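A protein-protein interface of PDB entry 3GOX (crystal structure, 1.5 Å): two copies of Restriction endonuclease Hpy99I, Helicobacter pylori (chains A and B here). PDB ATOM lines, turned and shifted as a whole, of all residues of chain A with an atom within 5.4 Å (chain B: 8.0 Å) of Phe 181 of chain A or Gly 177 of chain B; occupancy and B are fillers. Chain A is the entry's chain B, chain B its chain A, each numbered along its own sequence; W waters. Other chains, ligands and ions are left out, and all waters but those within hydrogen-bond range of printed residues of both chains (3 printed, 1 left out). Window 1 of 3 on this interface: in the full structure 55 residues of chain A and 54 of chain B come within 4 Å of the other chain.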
ATOM      1  N   GLY A 177      19.936  12.565   5.287  1.00  0.00           N
ATOM      2  CA  GLY A 177      19.418  12.295   3.951  1.00  0.00           C
ATOM      3  C   GLY A 177      18.375  11.200   3.983  1.00  0.00           C
ATOM      4  O   GLY A 177      17.331  11.315   3.323  1.00  0.00           O
ATOM      5  N   LEU A 178      18.643  10.107   4.707  1.00  0.00           N
ATOM      6  CA  LEU A 178      17.676   9.000   4.822  1.00  0.00           C
ATOM      7  C   LEU A 178      16.341   9.545   5.293  1.00  0.00           C
ATOM      8  O   LEU A 178      15.298   9.177   4.772  1.00  0.00           O
ATOM      9  CB  LEU A 178      18.147   7.908   5.796  1.00  0.00           C
ATOM     10  CG  LEU A 178      19.401   7.121   5.434  1.00  0.00           C
ATOM     11  CD1 LEU A 178      19.754   6.105   6.532  1.00  0.00           C
ATOM     12  CD2 LEU A 178      19.295   6.447   4.113  1.00  0.00           C
ATOM     13  N   GLY A 179      16.379  10.416   6.288  1.00  0.00           N
ATOM     14  CA  GLY A 179      15.162  10.959   6.876  1.00  0.00           C
ATOM     15  C   GLY A 179      14.351  11.795   5.913  1.00  0.00           C
ATOM     16  O   GLY A 179      13.126  11.806   5.989  1.00  0.00           O
ATOM     17  N   ARG A 180      15.019  12.515   5.020  1.00  0.00           N
ATOM     18  CA  ARG A 180      14.286  13.284   4.001  1.00  0.00           C
ATOM     19  C   ARG A 180      13.423  12.392   3.111  1.00  0.00           C
ATOM     20  O   ARG A 180      12.400  12.847   2.590  1.00  0.00           O
ATOM     21  CB  ARG A 180      15.247  14.127   3.175  1.00  0.00           C
ATOM     22  CG  ARG A 180      15.860  15.285   3.965  1.00  0.00           C
ATOM     23  CD  ARG A 180      17.117  15.769   3.307  1.00  0.00           C
ATOM     24  NE  ARG A 180      17.376  17.177   3.546  1.00  0.00           N
ATOM     25  CZ  ARG A 180      17.840  17.710   4.670  1.00  0.00           C
ATOM     26  NH1 ARG A 180      18.169  16.945   5.714  1.00  0.00           N
ATOM     27  NH2 ARG A 180      17.991  19.030   4.765  1.00  0.00           N
ATOM     28  N   PHE A 181      13.841  11.142   2.951  1.00  0.00           N
ATOM     29  CA  PHE A 181      13.122  10.157   2.153  1.00  0.00           C
ATOM     30  C   PHE A 181      12.444   9.099   3.022  1.00  0.00           C
ATOM     31  O   PHE A 181      12.105   8.014   2.566  1.00  0.00           O
ATOM     32  CB  PHE A 181      14.070   9.583   1.101  1.00  0.00           C
ATOM     33  CG  PHE A 181      14.705  10.657   0.277  1.00  0.00           C
ATOM     34  CD1 PHE A 181      13.906  11.535  -0.447  1.00  0.00           C
ATOM     35  CD2 PHE A 181      16.077  10.848   0.269  1.00  0.00           C
ATOM     36  CE1 PHE A 181      14.467  12.585  -1.164  1.00  0.00           C
ATOM     37  CE2 PHE A 181      16.646  11.870  -0.465  1.00  0.00           C
ATOM     38  CZ  PHE A 181      15.840  12.741  -1.188  1.00  0.00           C
ATOM     39  N   LYS A 182      12.177   9.476   4.270  1.00  0.00           N
ATOM     40  CA  LYS A 182      11.386   8.691   5.219  1.00  0.00           C
ATOM     41  C   LYS A 182      11.965   7.301   5.524  1.00  0.00           C
ATOM     42  O   LYS A 182      11.233   6.415   5.957  1.00  0.00           O
ATOM     43  CB  LYS A 182       9.925   8.596   4.748  1.00  0.00           C
ATOM     44  CG  LYS A 182       9.361   9.929   4.214  1.00  0.00           C
ATOM     45  CD  LYS A 182       7.858   9.857   3.911  1.00  0.00           C
ATOM     46  CE  LYS A 182       7.406  10.919   2.886  1.00  0.00           C
ATOM     47  NZ  LYS A 182       5.921  10.889   2.641  1.00  0.00           N
ATOM     48  N   ASP A 183      13.284   7.152   5.352  1.00  0.00           N
ATOM     49  CA  ASP A 183      13.965   5.850   5.517  1.00  0.00           C
ATOM     50  C   ASP A 183      13.286   4.741   4.686  1.00  0.00           C
ATOM     51  O   ASP A 183      13.293   3.577   5.086  1.00  0.00           O
ATOM     52  CB  ASP A 183      13.974   5.387   6.998  1.00  0.00           C
ATOM     53  CG  ASP A 183      14.856   6.221   7.924  1.00  0.00           C
ATOM     54  OD1 ASP A 183      15.362   7.313   7.567  1.00  0.00           O
ATOM     55  OD2 ASP A 183      15.043   5.744   9.071  1.00  0.00           O
ATOM     56  N   ASN A 184      12.690   5.109   3.554  1.00  0.00           N
ATOM     57  CA  ASN A 184      11.774   4.238   2.814  1.00  0.00           C
ATOM     58  C   ASN A 184      12.257   4.027   1.381  1.00  0.00           C
ATOM     59  O   ASN A 184      12.299   4.963   0.607  1.00  0.00           O
ATOM     60  CB  ASN A 184      10.386   4.884   2.795  1.00  0.00           C
ATOM     61  CG  ASN A 184       9.303   3.977   2.209  1.00  0.00           C
ATOM     62  OD1 ASN A 184       9.582   3.013   1.505  1.00  0.00           O
ATOM     63  ND2 ASN A 184       8.052   4.322   2.482  1.00  0.00           N
ATOM     64  N   PHE A 187      10.574   5.862  -1.740  1.00  0.00           N
ATOM     65  CA  PHE A 187      10.910   7.227  -2.128  1.00  0.00           C
ATOM     66  C   PHE A 187      12.308   7.305  -2.704  1.00  0.00           C
ATOM     67  O   PHE A 187      12.590   8.172  -3.516  1.00  0.00           O
ATOM     68  CB  PHE A 187      10.702   8.182  -0.956  1.00  0.00           C
ATOM     69  CG  PHE A 187       9.266   8.256  -0.526  1.00  0.00           C
ATOM     70  CD1 PHE A 187       8.309   8.811  -1.367  1.00  0.00           C
ATOM     71  CD2 PHE A 187       8.852   7.715   0.681  1.00  0.00           C
ATOM     72  CE1 PHE A 187       6.982   8.846  -1.003  1.00  0.00           C
ATOM     73  CE2 PHE A 187       7.508   7.745   1.053  1.00  0.00           C
ATOM     74  CZ  PHE A 187       6.576   8.311   0.208  1.00  0.00           C
ATOM     75  N   LEU A 188      13.187   6.388  -2.297  1.00  0.00           N
ATOM     76  CA  LEU A 188      14.511   6.324  -2.895  1.00  0.00           C
ATOM     77  C   LEU A 188      14.422   5.867  -4.356  1.00  0.00           C
ATOM     78  O   LEU A 188      15.143   6.374  -5.209  1.00  0.00           O
ATOM     79  CB  LEU A 188      15.434   5.416  -2.072  1.00  0.00           C
ATOM     80  CG  LEU A 188      15.772   5.972  -0.676  1.00  0.00           C
ATOM     81  CD1 LEU A 188      16.148   4.842   0.266  1.00  0.00           C
ATOM     82  CD2 LEU A 188      16.880   7.006  -0.758  1.00  0.00           C
ATOM     83  N   VAL A 191      13.382   8.817  -6.301  1.00  0.00           N
ATOM     84  CA  VAL A 191      14.530   9.675  -6.559  1.00  0.00           C
ATOM     85  C   VAL A 191      15.322   9.162  -7.767  1.00  0.00           C
ATOM     86  O   VAL A 191      15.715   9.943  -8.631  1.00  0.00           O
ATOM     87  CB  VAL A 191      15.473   9.761  -5.337  1.00  0.00           C
ATOM     88  CG1 VAL A 191      16.726  10.552  -5.683  1.00  0.00           C
ATOM     89  CG2 VAL A 191      14.769  10.408  -4.147  1.00  0.00           C
ATOM     90  N   CYS B 140       4.839  17.567  -3.727  1.00  0.00           N
ATOM     91  CA  CYS B 140       6.193  17.355  -4.233  1.00  0.00           C
ATOM     92  C   CYS B 140       6.282  16.058  -5.033  1.00  0.00           C
ATOM     93  O   CYS B 140       5.775  15.021  -4.608  1.00  0.00           O
ATOM     94  CB  CYS B 140       7.201  17.334  -3.083  1.00  0.00           C
ATOM     95  SG  CYS B 140       8.933  17.096  -3.604  1.00  0.00           S
ATOM     96  N   ILE B 142       8.675  14.088  -5.536  1.00  0.00           N
ATOM     97  CA  ILE B 142       9.585  13.082  -5.000  1.00  0.00           C
ATOM     98  C   ILE B 142       9.008  12.496  -3.718  1.00  0.00           C
ATOM     99  O   ILE B 142       8.588  11.336  -3.701  1.00  0.00           O
ATOM    100  CB  ILE B 142      11.009  13.632  -4.807  1.00  0.00           C
ATOM    101  CG1 ILE B 142      11.574  14.108  -6.152  1.00  0.00           C
ATOM    102  CG2 ILE B 142      11.928  12.554  -4.176  1.00  0.00           C
ATOM    103  CD1 ILE B 142      12.948  14.712  -6.076  1.00  0.00           C
ATOM    104  N   CYS B 143       8.912  13.313  -2.676  1.00  0.00           N
ATOM    105  CA  CYS B 143       8.448  12.850  -1.375  1.00  0.00           C
ATOM    106  C   CYS B 143       6.930  12.723  -1.262  1.00  0.00           C
ATOM    107  O   CYS B 143       6.444  12.149  -0.288  1.00  0.00           O
ATOM    108  CB  CYS B 143       8.962  13.758  -0.259  1.00  0.00           C
ATOM    109  SG  CYS B 143       8.246  15.413  -0.254  1.00  0.00           S
ATOM    110  N   LYS B 145       4.746  14.735  -0.393  1.00  0.00           N
ATOM    111  CA  LYS B 145       4.103  15.509   0.663  1.00  0.00           C
ATOM    112  C   LYS B 145       3.375  16.711   0.076  1.00  0.00           C
ATOM    113  O   LYS B 145       3.888  17.401  -0.799  1.00  0.00           O
ATOM    114  CB  LYS B 145       5.095  15.938   1.738  1.00  0.00           C
ATOM    115  CG  LYS B 145       5.788  14.762   2.413  1.00  0.00           C
ATOM    116  CD  LYS B 145       6.406  15.148   3.786  1.00  0.00           C
ATOM    117  CE  LYS B 145       7.476  16.244   3.722  1.00  0.00           C
ATOM    118  NZ  LYS B 145       8.738  15.816   2.988  1.00  0.00           N
ATOM    119  N   ILE B 170      10.751  21.128  -6.860  1.00  0.00           N
ATOM    120  CA  ILE B 170      10.679  20.149  -5.779  1.00  0.00           C
ATOM    121  C   ILE B 170      10.857  20.895  -4.447  1.00  0.00           C
ATOM    122  O   ILE B 170      11.296  22.056  -4.414  1.00  0.00           O
ATOM    123  CB  ILE B 170      11.752  19.010  -5.913  1.00  0.00           C
ATOM    124  CG1 ILE B 170      13.184  19.561  -5.863  1.00  0.00           C
ATOM    125  CG2 ILE B 170      11.532  18.190  -7.202  1.00  0.00           C
ATOM    126  CD1 ILE B 170      14.260  18.463  -5.887  1.00  0.00           C
ATOM    127  N   CYS B 171      10.550  20.233  -3.334  1.00  0.00           N
ATOM    128  CA  CYS B 171      10.744  20.875  -2.032  1.00  0.00           C
ATOM    129  C   CYS B 171      12.231  20.934  -1.664  1.00  0.00           C
ATOM    130  O   CYS B 171      13.030  20.128  -2.125  1.00  0.00           O
ATOM    131  CB  CYS B 171       9.882  20.220  -0.943  1.00  0.00           C
ATOM    132  SG  CYS B 171      10.511  18.639  -0.304  1.00  0.00           S
ATOM    133  N   ASP B 172      12.576  21.936  -0.867  1.00  0.00           N
ATOM    134  CA  ASP B 172      13.964  22.163  -0.410  1.00  0.00           C
ATOM    135  C   ASP B 172      14.482  20.952   0.359  1.00  0.00           C
ATOM    136  O   ASP B 172      15.656  20.612   0.248  1.00  0.00           O
ATOM    137  CB  ASP B 172      14.003  23.450   0.445  1.00  0.00           C
ATOM    138  CG  ASP B 172      15.397  23.786   0.993  1.00  0.00           C
ATOM    139  OD1 ASP B 172      16.209  24.374   0.262  1.00  0.00           O
ATOM    140  OD2 ASP B 172      15.642  23.539   2.199  1.00  0.00           O
ATOM    141  N   SER B 173      13.617  20.300   1.120  1.00  0.00           N
ATOM    142  CA  SER B 173      14.010  19.091   1.855  1.00  0.00           C
ATOM    143  C   SER B 173      14.518  18.021   0.891  1.00  0.00           C
ATOM    144  O   SER B 173      15.611  17.455   1.079  1.00  0.00           O
ATOM    145  CB  SER B 173      12.817  18.595   2.660  1.00  0.00           C
ATOM    146  OG  SER B 173      13.071  17.388   3.334  1.00  0.00           O
ATOM    147  N   CYS B 174      13.751  17.719  -0.149  1.00  0.00           N
ATOM    148  CA  CYS B 174      14.170  16.737  -1.153  1.00  0.00           C
ATOM    149  C   CYS B 174      15.420  17.177  -1.894  1.00  0.00           C
ATOM    150  O   CYS B 174      16.309  16.365  -2.138  1.00  0.00           O
ATOM    151  CB  CYS B 174      13.040  16.473  -2.159  1.00  0.00           C
ATOM    152  SG  CYS B 174      11.763  15.388  -1.457  1.00  0.00           S
ATOM    153  N   ASN B 175      15.494  18.450  -2.262  1.00  0.00           N
ATOM    154  CA  ASN B 175      16.633  18.954  -3.020  1.00  0.00           C
ATOM    155  C   ASN B 175      17.946  18.790  -2.236  1.00  0.00           C
ATOM    156  O   ASN B 175      18.964  18.356  -2.788  1.00  0.00           O
ATOM    157  CB  ASN B 175      16.423  20.419  -3.394  1.00  0.00           C
ATOM    158  CG  ASN B 175      17.481  20.930  -4.342  1.00  0.00           C
ATOM    159  OD1 ASN B 175      17.677  20.373  -5.411  1.00  0.00           O
ATOM    160  ND2 ASN B 175      18.165  22.005  -3.957  1.00  0.00           N
ATOM    161  N   THR B 176      17.896  19.107  -0.949  1.00  0.00           N
ATOM    162  CA  THR B 176      19.072  19.003  -0.097  1.00  0.00           C
ATOM    163  C   THR B 176      19.367  17.548   0.281  1.00  0.00           C
ATOM    164  O   THR B 176      20.482  17.236   0.708  1.00  0.00           O
ATOM    165  CB  THR B 176      18.951  19.918   1.130  1.00  0.00           C
ATOM    166  OG1 THR B 176      17.728  19.677   1.841  1.00  0.00           O
ATOM    167  CG2 THR B 176      19.040  21.380   0.689  1.00  0.00           C
ATOM    168  N   GLY B 177      18.390  16.660   0.103  1.00  0.00           N
ATOM    169  CA  GLY B 177      18.602  15.219   0.178  1.00  0.00           C
ATOM    170  C   GLY B 177      19.312  14.662  -1.046  1.00  0.00           C
ATOM    171  O   GLY B 177      20.223  13.826  -0.924  1.00  0.00           O
ATOM    172  N   LEU B 178      18.910  15.090  -2.244  1.00  0.00           N
ATOM    173  CA  LEU B 178      19.595  14.690  -3.481  1.00  0.00           C
ATOM    174  C   LEU B 178      21.082  14.975  -3.356  1.00  0.00           C
ATOM    175  O   LEU B 178      21.910  14.152  -3.749  1.00  0.00           O
ATOM    176  CB  LEU B 178      19.051  15.459  -4.700  1.00  0.00           C
ATOM    177  CG  LEU B 178      17.579  15.260  -5.061  1.00  0.00           C
ATOM    178  CD1 LEU B 178      17.208  16.050  -6.311  1.00  0.00           C
ATOM    179  CD2 LEU B 178      17.262  13.832  -5.233  1.00  0.00           C
ATOM    180  N   GLY B 179      21.433  16.146  -2.838  1.00  0.00           N
ATOM    181  CA  GLY B 179      22.847  16.535  -2.745  1.00  0.00           C
ATOM    182  C   GLY B 179      23.664  15.697  -1.781  1.00  0.00           C
ATOM    183  O   GLY B 179      24.876  15.474  -1.986  1.00  0.00           O
ATOM    184  N   ARG B 180      23.023  15.247  -0.706  1.00  0.00           N
ATOM    185  CA  ARG B 180      23.720  14.342   0.222  1.00  0.00           C
ATOM    186  C   ARG B 180      24.217  13.072  -0.479  1.00  0.00           C
ATOM    187  O   ARG B 180      25.213  12.473  -0.078  1.00  0.00           O
ATOM    188  CB  ARG B 180      22.817  13.990   1.376  1.00  0.00           C
ATOM    189  CG  ARG B 180      22.671  15.153   2.357  1.00  0.00           C
ATOM    190  CD  ARG B 180      21.472  15.005   3.277  1.00  0.00           C
ATOM    191  NE  ARG B 180      21.612  15.696   4.547  1.00  0.00           N
ATOM    192  CZ  ARG B 180      21.457  17.006   4.737  1.00  0.00           C
ATOM    193  NH1 ARG B 180      21.146  17.803   3.717  1.00  0.00           N
ATOM    194  NH2 ARG B 180      21.635  17.526   5.946  1.00  0.00           N
ATOM    195  N   PHE B 181      23.498  12.664  -1.519  1.00  0.00           N
ATOM    196  CA  PHE B 181      23.824  11.469  -2.304  1.00  0.00           C
ATOM    197  C   PHE B 181      24.377  11.827  -3.683  1.00  0.00           C
ATOM    198  O   PHE B 181      24.370  11.011  -4.603  1.00  0.00           O
ATOM    199  CB  PHE B 181      22.589  10.550  -2.355  1.00  0.00           C
ATOM    200  CG  PHE B 181      22.064  10.216  -0.975  1.00  0.00           C
ATOM    201  CD1 PHE B 181      22.899   9.622  -0.032  1.00  0.00           C
ATOM    202  CD2 PHE B 181      20.781  10.554  -0.597  1.00  0.00           C
ATOM    203  CE1 PHE B 181      22.451   9.351   1.255  1.00  0.00           C
ATOM    204  CE2 PHE B 181      20.327  10.278   0.691  1.00  0.00           C
ATOM    205  CZ  PHE B 181      21.163   9.665   1.615  1.00  0.00           C
ATOM    206  N   LYS B 182      24.889  13.057  -3.791  1.00  0.00           N
ATOM    207  CA  LYS B 182      25.654  13.540  -4.950  1.00  0.00           C
ATOM    208  C   LYS B 182      24.833  13.552  -6.244  1.00  0.00           C
ATOM    209  O   LYS B 182      25.397  13.504  -7.332  1.00  0.00           O
ATOM    210  CB  LYS B 182      26.952  12.734  -5.127  1.00  0.00           C
ATOM    211  CG  LYS B 182      27.721  12.491  -3.824  1.00  0.00           C
ATOM    212  CD  LYS B 182      29.012  11.692  -4.033  1.00  0.00           C
ATOM    213  CE  LYS B 182      29.452  10.942  -2.755  1.00  0.00           C
ATOM    214  NZ  LYS B 182      30.819  10.313  -2.879  1.00  0.00           N
ATOM    215  N   ASP B 183      23.510  13.652  -6.111  1.00  0.00           N
ATOM    216  CA  ASP B 183      22.597  13.598  -7.270  1.00  0.00           C
ATOM    217  C   ASP B 183      22.874  12.361  -8.136  1.00  0.00           C
ATOM    218  O   ASP B 183      22.663  12.386  -9.353  1.00  0.00           O
ATOM    219  CB  ASP B 183      22.716  14.857  -8.168  1.00  0.00           C
ATOM    220  CG  ASP B 183      22.237  16.139  -7.504  1.00  0.00           C
ATOM    221  OD1 ASP B 183      21.964  16.176  -6.286  1.00  0.00           O
ATOM    222  OD2 ASP B 183      22.164  17.156  -8.237  1.00  0.00           O
ATOM    223  N   ASN B 184      23.337  11.277  -7.516  1.00  0.00           N
ATOM    224  CA  ASN B 184      23.901  10.140  -8.253  1.00  0.00           C
ATOM    225  C   ASN B 184      23.139   8.868  -7.897  1.00  0.00           C
ATOM    226  O   ASN B 184      23.137   8.458  -6.746  1.00  0.00           O
ATOM    227  CB  ASN B 184      25.391  10.006  -7.931  1.00  0.00           C
ATOM    228  CG  ASN B 184      26.086   8.954  -8.773  1.00  0.00           C
ATOM    229  OD1 ASN B 184      25.447   8.079  -9.356  1.00  0.00           O
ATOM    230  ND2 ASN B 184      27.405   9.037  -8.837  1.00  0.00           N
ATOM    231  N   LEU B 188      22.098   6.277  -4.350  1.00  0.00           N
ATOM    232  CA  LEU B 188      20.716   5.994  -3.979  1.00  0.00           C
ATOM    233  C   LEU B 188      20.481   4.490  -3.933  1.00  0.00           C
ATOM    234  O   LEU B 188      19.794   3.987  -3.043  1.00  0.00           O
ATOM    235  CB  LEU B 188      19.754   6.661  -4.961  1.00  0.00           C
ATOM    236  CG  LEU B 188      19.824   8.193  -4.922  1.00  0.00           C
ATOM    237  CD1 LEU B 188      19.084   8.728  -6.127  1.00  0.00           C
ATOM    238  CD2 LEU B 188      19.267   8.743  -3.622  1.00  0.00           C
ATOM    239  N   VAL B 191      21.834   3.264  -0.815  1.00  0.00           N
ATOM    240  CA  VAL B 191      20.893   3.518   0.273  1.00  0.00           C
ATOM    241  C   VAL B 191      19.804   2.439   0.328  1.00  0.00           C
ATOM    242  O   VAL B 191      19.466   1.943   1.395  1.00  0.00           O
ATOM    243  CB  VAL B 191      20.203   4.886   0.144  1.00  0.00           C
ATOM    244  CG1 VAL B 191      19.175   5.053   1.249  1.00  0.00           C
ATOM    245  CG2 VAL B 191      21.219   6.041   0.180  1.00  0.00           C
ATOM    246  N   LEU B 195      19.119  -0.096   3.465  1.00  0.00           N
ATOM    247  CA  LEU B 195      17.835  -0.125   4.183  1.00  0.00           C
ATOM    248  C   LEU B 195      17.215  -1.522   4.151  1.00  0.00           C
ATOM    249  O   LEU B 195      16.817  -2.064   5.191  1.00  0.00           O
ATOM    250  CB  LEU B 195      16.847   0.888   3.595  1.00  0.00           C
ATOM    251  CG  LEU B 195      17.176   2.377   3.742  1.00  0.00           C
ATOM    252  CD1 LEU B 195      16.198   3.241   2.953  1.00  0.00           C
ATOM    253  CD2 LEU B 195      17.208   2.809   5.205  1.00  0.00           C
HETATM  254  O   HOH W   1      15.672  21.262   3.899  1.00  0.00           O
HETATM  255  O   HOH W   2      11.917  15.461   1.806  1.00  0.00           O
HETATM  256  O   HOH W   3       9.845  13.440   3.968  1.00  0.00           O
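O of Cys 143 of chain B lies within hydrogen-bond range of NZ of Lys 182 of chain A (3.2 Å). The backbone carbonyl oxygen (O) of Ser 173 of chain B is in hydrogen-bond range of the guanidinium group (NE) of Arg 180 of chain A (3.0 Å). OG1 of Thr 176 of chain B lies within hydrogen-bond range of NH2 of Arg 180 of chain A, 3.0 Å away.
The side-chain sulfur (SG) of Cys 140 of chain B lies close to the backbone NH (N) of Ile 142 of chain B, at 3.6 Å. N of Cys 140 of chain B lies within hydrogen-bond range of O of Lys 145 of chain B, at 3.1 Å. NZ of Lys 145 of chain B lies close to SG of Cys 143 of chain B (3.3 Å). The side-chain sulfur of Cys 171 of chain B lies close to the backbone NH of Ser 173 of chain B, 3.8 Å away. O of Ser 173 of chain B lies within hydrogen-bond range of OG1 of Thr 176 of chain B, at 3.2 Å. O of Thr 176 of chain B lies within hydrogen-bond range of NH1 of Arg 180 of chain B (3.1 Å).
Among the printed residues, pairs that only touch across the chains: Val 191 of chain A with Leu 188 of chain B, Leu 188 of chain A with Leu 195 of chain B, Leu 178 of chain A with Val 191 of chain B, Leu 188 of chain A with Val 191 of chain B, Val 191 of chain A with Leu 178 of chain B, Phe 187 of chain A with Cys 143 of chain B, Arg 180 of chain A with Arg 180 of chain B, Phe 187 of chain A with Ile 142 of chain B, Gly 177 of chain A with Arg 180 of chain B, Arg 180 of chain A with Gly 177 of chain B, Val 191 of chain A with Ile 142 of chain B, Asp 183 of chain A with Leu 195 of chain B, Phe 181 of chain A with Cys 174 of chain B, Lys 182 of chain A with Lys 145 of chain B, Phe 181 of chain A with Gly 177 of chain B, Gly 177 of chain A with Phe 181 of chain B and Phe 181 of chain A with Ile 142 of chain B.
Gly 177 of chain B touches just these residues of chain A: Arg 180 (3.5 Å) and Phe 181 (3.9 Å). Printed residues of chain A within 4 Å of Lys 145 of chain B: Lys 182. Of the printed residues of chain A, Ser 173 of chain B touches Arg 180. Gly 179 of chain A touches none of the printed residues of chain B. The nearest residue of chain A that does not touch Gly 177 of chain B is Gly 177 of chain A (4.8 Å).
Hydrophobic or aromatic side chains of chain B within 4 Å of the printed part of chain A: Ile 142, Leu 178, Phe 181, Leu 188, Val 191 and Leu 195. Of the 11 printed residues of chain A, 9 touch a printed residue of chain B. Hydrophobic or aromatic side chains of chain A that line the printed part of chain B: Leu 178, Phe 181, Phe 187, Leu 188 and Val 191. Among the printed residues, 20 pairs touch across the chains. Among the printed residues, no Asp or Glu carboxylate lies within 4 Å of a Lys or Arg side-chain nitrogen of the other chain.
Gly 177 of chain A touches Arg 180 of chain B, and with the chains exchanged Arg 180 of chain A touches Gly 177 of chain B. Leu 178 of chain A touches Val 191 of chain B, and with the chains exchanged Val 191 of chain A touches Leu 178 of chain B. Arg 180 of chain B touches its own counterpart, Arg 180 of chain A. Leu 188 of chain A touches Val 191 of chain B, and with the chains exchanged Val 191 of chain A touches Leu 188 of chain B. Of the 20 pairs that touch across the chains among the printed residues, 9 have their exchanged pair printed and touching as well.
Water W2 lies within hydrogen-bond range of OG of Ser 173 of chain B, O of Arg 180 of chain A and NZ of Lys 145 of chain B. Water W3 lies within hydrogen-bond range of the side-chain amino group of Lys 145 of chain B (2.8 Å) and the backbone carbonyl oxygen of Arg 180 of chain A (3.0 Å). Water W1 lies within hydrogen-bond range of OD2 of Asp 172 of chain B, OG1 of Thr 176 of chain B and NH2 of Arg 180 of chain A.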
